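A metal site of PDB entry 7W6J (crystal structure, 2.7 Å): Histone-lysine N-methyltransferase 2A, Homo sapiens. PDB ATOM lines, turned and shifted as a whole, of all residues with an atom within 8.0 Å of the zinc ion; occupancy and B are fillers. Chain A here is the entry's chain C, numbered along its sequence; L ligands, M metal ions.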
ATOM      1  N   ILE A  27      -0.621  -2.137  22.189  1.00  0.00           N
ATOM      2  CA  ILE A  27      -0.066  -0.805  22.401  1.00  0.00           C
ATOM      3  C   ILE A  27      -0.635   0.172  21.391  1.00  0.00           C
ATOM      4  O   ILE A  27      -1.244   1.190  21.754  1.00  0.00           O
ATOM      5  CB  ILE A  27       1.468  -0.846  22.343  1.00  0.00           C
ATOM      6  CG1 ILE A  27       2.036  -1.555  23.582  1.00  0.00           C
ATOM      7  CG2 ILE A  27       2.047   0.555  22.232  1.00  0.00           C
ATOM      8  CD1 ILE A  27       3.544  -1.699  23.562  1.00  0.00           C
ATOM      9  N   HIS A  97       6.735   1.968  20.594  1.00  0.00           N
ATOM     10  CA  HIS A  97       7.532   2.531  21.671  1.00  0.00           C
ATOM     11  C   HIS A  97       7.041   2.012  23.011  1.00  0.00           C
ATOM     12  O   HIS A  97       5.849   1.727  23.194  1.00  0.00           O
ATOM     13  CB  HIS A  97       7.477   4.065  21.647  1.00  0.00           C
ATOM     14  CG  HIS A  97       7.888   4.704  22.936  1.00  0.00           C
ATOM     15  ND1 HIS A  97       9.135   5.269  23.128  1.00  0.00           N
ATOM     16  CD2 HIS A  97       7.226   4.886  24.100  1.00  0.00           C
ATOM     17  CE1 HIS A  97       9.217   5.761  24.343  1.00  0.00           C
ATOM     18  NE2 HIS A  97       8.072   5.541  24.959  1.00  0.00           N
ATOM     19  N   SER A  98       7.968   1.882  23.949  1.00  0.00           N
ATOM     20  CA  SER A  98       7.619   1.562  25.321  1.00  0.00           C
ATOM     21  C   SER A  98       8.483   2.395  26.247  1.00  0.00           C
ATOM     22  O   SER A  98       9.685   2.564  26.000  1.00  0.00           O
ATOM     23  CB  SER A  98       7.811   0.074  25.616  1.00  0.00           C
ATOM     24  OG  SER A  98       7.417  -0.244  26.948  1.00  0.00           O
ATOM     25  N   CYS A  99       7.876   2.913  27.305  1.00  0.00           N
ATOM     26  CA  CYS A  99       8.665   3.495  28.391  1.00  0.00           C
ATOM     27  C   CYS A  99       9.423   2.479  29.232  1.00  0.00           C
ATOM     28  O   CYS A  99      10.306   2.911  29.963  1.00  0.00           O
ATOM     29  CB  CYS A  99       7.787   4.329  29.335  1.00  0.00           C
ATOM     30  SG  CYS A  99       6.675   5.393  28.518  1.00  0.00           S
ATOM     31  N   GLU A 100       9.092   1.166  29.220  1.00  0.00           N
ATOM     32  CA  GLU A 100       9.871   0.137  29.931  1.00  0.00           C
ATOM     33  C   GLU A 100      10.118  -0.987  28.930  1.00  0.00           C
ATOM     34  O   GLU A 100       9.596  -2.099  29.069  1.00  0.00           O
ATOM     35  CB  GLU A 100       9.155  -0.368  31.179  1.00  0.00           C
ATOM     36  CG  GLU A 100       9.960  -1.146  32.237  1.00  0.00           C
ATOM     37  CD  GLU A 100       9.078  -1.330  33.478  1.00  0.00           C
ATOM     38  OE1 GLU A 100       7.837  -1.177  33.347  1.00  0.00           O
ATOM     39  OE2 GLU A 100       9.644  -1.289  34.546  1.00  0.00           O
ATOM     40  N   PRO A 146       0.313  11.084  22.961  1.00  0.00           N
ATOM     41  CA  PRO A 146       0.470  10.322  24.207  1.00  0.00           C
ATOM     42  C   PRO A 146       1.012   8.915  23.974  1.00  0.00           C
ATOM     43  O   PRO A 146       1.105   8.419  22.848  1.00  0.00           O
ATOM     44  CB  PRO A 146      -0.970  10.265  24.757  1.00  0.00           C
ATOM     45  CG  PRO A 146      -1.724  11.328  23.990  1.00  0.00           C
ATOM     46  CD  PRO A 146      -1.103  11.307  22.639  1.00  0.00           C
ATOM     47  N   CYS A 147       1.345   8.272  25.089  1.00  0.00           N
ATOM     48  CA  CYS A 147       1.886   6.922  25.086  1.00  0.00           C
ATOM     49  C   CYS A 147       0.867   5.962  25.703  1.00  0.00           C
ATOM     50  O   CYS A 147       0.199   6.294  26.683  1.00  0.00           O
ATOM     51  CB  CYS A 147       3.207   6.854  25.855  1.00  0.00           C
ATOM     52  SG  CYS A 147       3.951   5.211  25.895  1.00  0.00           S
ATOM     53  N   ASN A 148       0.755   4.773  25.103  1.00  0.00           N
ATOM     54  CA  ASN A 148      -0.153   3.732  25.559  1.00  0.00           C
ATOM     55  C   ASN A 148       0.617   2.408  25.480  1.00  0.00           C
ATOM     56  O   ASN A 148       0.250   1.464  24.789  1.00  0.00           O
ATOM     57  CB  ASN A 148      -1.441   3.774  24.737  1.00  0.00           C
ATOM     58  CG  ASN A 148      -2.432   2.658  25.101  1.00  0.00           C
ATOM     59  OD1 ASN A 148      -2.299   1.509  24.694  1.00  0.00           O
ATOM     60  ND2 ASN A 148      -3.443   3.019  25.898  1.00  0.00           N
ATOM     61  N   CYS A 149       1.756   2.363  26.169  1.00  0.00           N
ATOM     62  CA  CYS A 149       2.555   1.150  26.230  1.00  0.00           C
ATOM     63  C   CYS A 149       2.132   0.213  27.352  1.00  0.00           C
ATOM     64  O   CYS A 149       2.515  -0.956  27.341  1.00  0.00           O
ATOM     65  CB  CYS A 149       4.042   1.507  26.396  1.00  0.00           C
ATOM     66  SG  CYS A 149       4.458   2.219  28.001  1.00  0.00           S
ATOM     67  N   GLY A 150       1.335   0.707  28.307  1.00  0.00           N
ATOM     68  CA  GLY A 150       0.881  -0.109  29.408  1.00  0.00           C
ATOM     69  C   GLY A 150       1.897  -0.347  30.498  1.00  0.00           C
ATOM     70  O   GLY A 150       1.570  -1.025  31.480  1.00  0.00           O
ATOM     71  N   ALA A 151       3.110   0.186  30.364  1.00  0.00           N
ATOM     72  CA  ALA A 151       4.122   0.021  31.401  1.00  0.00           C
ATOM     73  C   ALA A 151       3.696   0.738  32.673  1.00  0.00           C
ATOM     74  O   ALA A 151       3.105   1.830  32.629  1.00  0.00           O
ATOM     75  CB  ALA A 151       5.471   0.554  30.919  1.00  0.00           C
ATOM     76  N   LYS A 152       3.994   0.123  33.813  1.00  0.00           N
ATOM     77  CA  LYS A 152       3.606   0.700  35.096  1.00  0.00           C
ATOM     78  C   LYS A 152       4.374   1.976  35.428  1.00  0.00           C
ATOM     79  O   LYS A 152       3.977   2.683  36.350  1.00  0.00           O
ATOM     80  CB  LYS A 152       3.792  -0.334  36.204  1.00  0.00           C
ATOM     81  CG  LYS A 152       2.597  -1.260  36.372  1.00  0.00           C
ATOM     82  CD  LYS A 152       3.029  -2.688  36.669  1.00  0.00           C
ATOM     83  CE  LYS A 152       3.718  -2.781  38.014  1.00  0.00           C
ATOM     84  NZ  LYS A 152       2.749  -2.649  39.143  1.00  0.00           N
ATOM     85  N   LYS A 153       5.448   2.272  34.700  1.00  0.00           N
ATOM     86  CA  LYS A 153       6.157   3.527  34.871  1.00  0.00           C
ATOM     87  C   LYS A 153       6.152   4.303  33.560  1.00  0.00           C
ATOM     88  O   LYS A 153       7.191   4.793  33.107  1.00  0.00           O
ATOM     89  CB  LYS A 153       7.578   3.283  35.383  1.00  0.00           C
ATOM     90  CG  LYS A 153       7.610   2.478  36.676  1.00  0.00           C
ATOM     91  CD  LYS A 153       8.967   2.535  37.350  1.00  0.00           C
ATOM     92  CE  LYS A 153       8.917   1.837  38.697  1.00  0.00           C
ATOM     93  NZ  LYS A 153      10.139   2.067  39.503  1.00  0.00           N
ATOM     94  N   CYS A 154       4.975   4.403  32.947  1.00  0.00           N
ATOM     95  CA  CYS A 154       4.851   5.028  31.642  1.00  0.00           C
ATOM     96  C   CYS A 154       4.931   6.544  31.752  1.00  0.00           C
ATOM     97  O   CYS A 154       4.261   7.145  32.585  1.00  0.00           O
ATOM     98  CB  CYS A 154       3.527   4.609  31.002  1.00  0.00           C
ATOM     99  SG  CYS A 154       3.064   5.503  29.505  1.00  0.00           S
ATOM    100  N   ARG A 155       5.770   7.156  30.914  1.00  0.00           N
ATOM    101  CA  ARG A 155       5.900   8.610  30.903  1.00  0.00           C
ATOM    102  C   ARG A 155       4.640   9.305  30.400  1.00  0.00           C
ATOM    103  O   ARG A 155       4.503  10.514  30.619  1.00  0.00           O
ATOM    104  CB  ARG A 155       7.093   9.025  30.033  1.00  0.00           C
ATOM    105  CG  ARG A 155       8.416   8.377  30.407  1.00  0.00           C
ATOM    106  CD  ARG A 155       9.529   8.942  29.543  1.00  0.00           C
ATOM    107  NE  ARG A 155       9.270   8.681  28.117  1.00  0.00           N
ATOM    108  CZ  ARG A 155      10.153   8.910  27.148  1.00  0.00           C
ATOM    109  NH1 ARG A 155       9.826   8.650  25.890  1.00  0.00           N
ATOM    110  NH2 ARG A 155      11.350   9.389  27.438  1.00  0.00           N
ATOM    111  N   LYS A 156       3.762   8.579  29.723  1.00  0.00           N
ATOM    112  CA  LYS A 156       2.448   8.963  29.220  1.00  0.00           C
ATOM    113  C   LYS A 156       2.534   9.720  27.895  1.00  0.00           C
ATOM    114  O   LYS A 156       1.516   9.904  27.228  1.00  0.00           O
ATOM    115  CB  LYS A 156       1.610   9.773  30.238  1.00  0.00           C
ATOM    116  CG  LYS A 156       0.155   9.910  29.850  1.00  0.00           C
ATOM    117  CD  LYS A 156      -0.454   8.517  29.814  1.00  0.00           C
ATOM    118  CE  LYS A 156      -1.886   8.540  29.304  1.00  0.00           C
ATOM    119  NZ  LYS A 156      -2.422   7.154  29.172  1.00  0.00           N
ATOM    120  N   PHE A 157       3.724  10.159  27.466  1.00  0.00           N
ATOM    121  CA  PHE A 157       3.891  10.785  26.165  1.00  0.00           C
ATOM    122  C   PHE A 157       5.100  10.209  25.465  1.00  0.00           C
ATOM    123  O   PHE A 157       6.111   9.876  26.102  1.00  0.00           O
ATOM    124  CB  PHE A 157       4.042  12.311  26.285  1.00  0.00           C
ATOM    125  CG  PHE A 157       2.864  12.991  26.926  1.00  0.00           C
ATOM    126  CD1 PHE A 157       1.734  13.280  26.180  1.00  0.00           C
ATOM    127  CD2 PHE A 157       2.890  13.346  28.257  1.00  0.00           C
ATOM    128  CE1 PHE A 157       0.645  13.913  26.763  1.00  0.00           C
ATOM    129  CE2 PHE A 157       1.809  13.980  28.847  1.00  0.00           C
ATOM    130  CZ  PHE A 157       0.685  14.259  28.092  1.00  0.00           C
ATOM    131  N   LEU A 158       5.001  10.073  24.136  1.00  0.00           N
ATOM    132  CA  LEU A 158       6.162   9.692  23.350  1.00  0.00           C
ATOM    133  C   LEU A 158       7.151  10.836  23.200  1.00  0.00           C
ATOM    134  O   LEU A 158       8.324  10.598  22.890  1.00  0.00           O
ATOM    135  CB  LEU A 158       5.744   9.178  21.970  1.00  0.00           C
ATOM    136  CG  LEU A 158       4.693   8.056  21.904  1.00  0.00           C
ATOM    137  CD1 LEU A 158       4.130   7.833  20.506  1.00  0.00           C
ATOM    138  CD2 LEU A 158       5.257   6.777  22.423  1.00  0.00           C
HETATM  139  N1  LIG L   1       2.250   0.968  15.163  1.00  0.00           N
HETATM  140  C1  LIG L   1       2.335   1.398  13.778  1.00  0.00           C
HETATM  141  C2  LIG L   1       3.773   1.272  13.280  1.00  0.00           C
HETATM  142  C3  LIG L   1       4.806   1.935  14.186  1.00  0.00           C
HETATM  143  S1  LIG L   1       5.247   3.584  13.579  1.00  0.00           S
HETATM  144  C4  LIG L   1       1.409   0.595  12.865  1.00  0.00           C
HETATM  145  O1  LIG L   1       0.578  -0.186  13.338  1.00  0.00           O
HETATM  146  O2  LIG L   1       1.463   0.715  11.648  1.00  0.00           O
HETATM  147  C5  LIG L   1       4.935   4.261  15.218  1.00  0.00           C
HETATM  148  C6  LIG L   1       3.557   4.889  15.343  1.00  0.00           C
HETATM  149  O3  LIG L   1       2.835   4.208  16.348  1.00  0.00           O
HETATM  150  C7  LIG L   1       3.661   6.360  15.740  1.00  0.00           C
HETATM  151  O4  LIG L   1       3.039   7.173  14.780  1.00  0.00           O
HETATM  152  C8  LIG L   1       2.946   6.472  17.066  1.00  0.00           C
HETATM  153  O5  LIG L   1       1.871   7.375  16.968  1.00  0.00           O
HETATM  154  C9  LIG L   1       2.421   5.080  17.373  1.00  0.00           C
HETATM  155  N2  LIG L   1       2.989   4.609  18.653  1.00  0.00           N
HETATM  156  C10 LIG L   1       4.264   4.142  18.835  1.00  0.00           C
HETATM  157  N3  LIG L   1       4.414   3.808  20.141  1.00  0.00           N
HETATM  158  C11 LIG L   1       3.253   4.058  20.784  1.00  0.00           C
HETATM  159  C12 LIG L   1       2.872   3.890  22.110  1.00  0.00           C
HETATM  160  N4  LIG L   1       3.729   3.402  23.003  1.00  0.00           N
HETATM  161  N5  LIG L   1       1.596   4.235  22.482  1.00  0.00           N
HETATM  162  C13 LIG L   1       0.701   4.745  21.557  1.00  0.00           C
HETATM  163  N6  LIG L   1       1.090   4.902  20.237  1.00  0.00           N
HETATM  164  C14 LIG L   1       2.345   4.557  19.859  1.00  0.00           C
HETATM  165 ZN    ZN M   1       4.570   4.542  28.027  1.00  0.00          ZN
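Within 4 Å of the zinc ion: Cys 99, Cys 147, Cys 149 and Cys 154. The nearest printed residue that does not touch the zinc ion is Arg 155 (4.1 Å).
A nitrogen (N4) of the ligand lies close to the side-chain sulfur (SG) of Cys 147 (3.4 Å). The backbone NH (N) of His 97 lies within hydrogen-bond range of a nitrogen (N3) of the ligand (3.0 Å). N of Asn 148 sits at hydrogen-bond distance from N5 of the ligand, at 2.8 Å. A nitrogen (N4) of the ligand is in hydrogen-bond range of the backbone carbonyl oxygen (O) of His 97 (2.7 Å).
The backbone NH (N) of Ala 151 sits close to the side-chain sulfur (SG) of Cys 149 (3.4 Å). The side-chain sulfur (SG) of Cys 99 lies close to the backbone NH (N) of Arg 155 (3.1 Å). N of Lys 156 lies close to SG of Cys 154, 3.2 Å away. N of Cys 147 is in hydrogen-bond range of O of Lys 156, 2.7 Å away.
The zinc ion is bound by the side-chain sulfur of Cys 147 (2.3 Å), the side-chain sulfur of Cys 154 (2.3 Å), the side-chain sulfur of Cys 99 (2.3 Å) and the side-chain sulfur of Cys 149 (2.3 Å).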
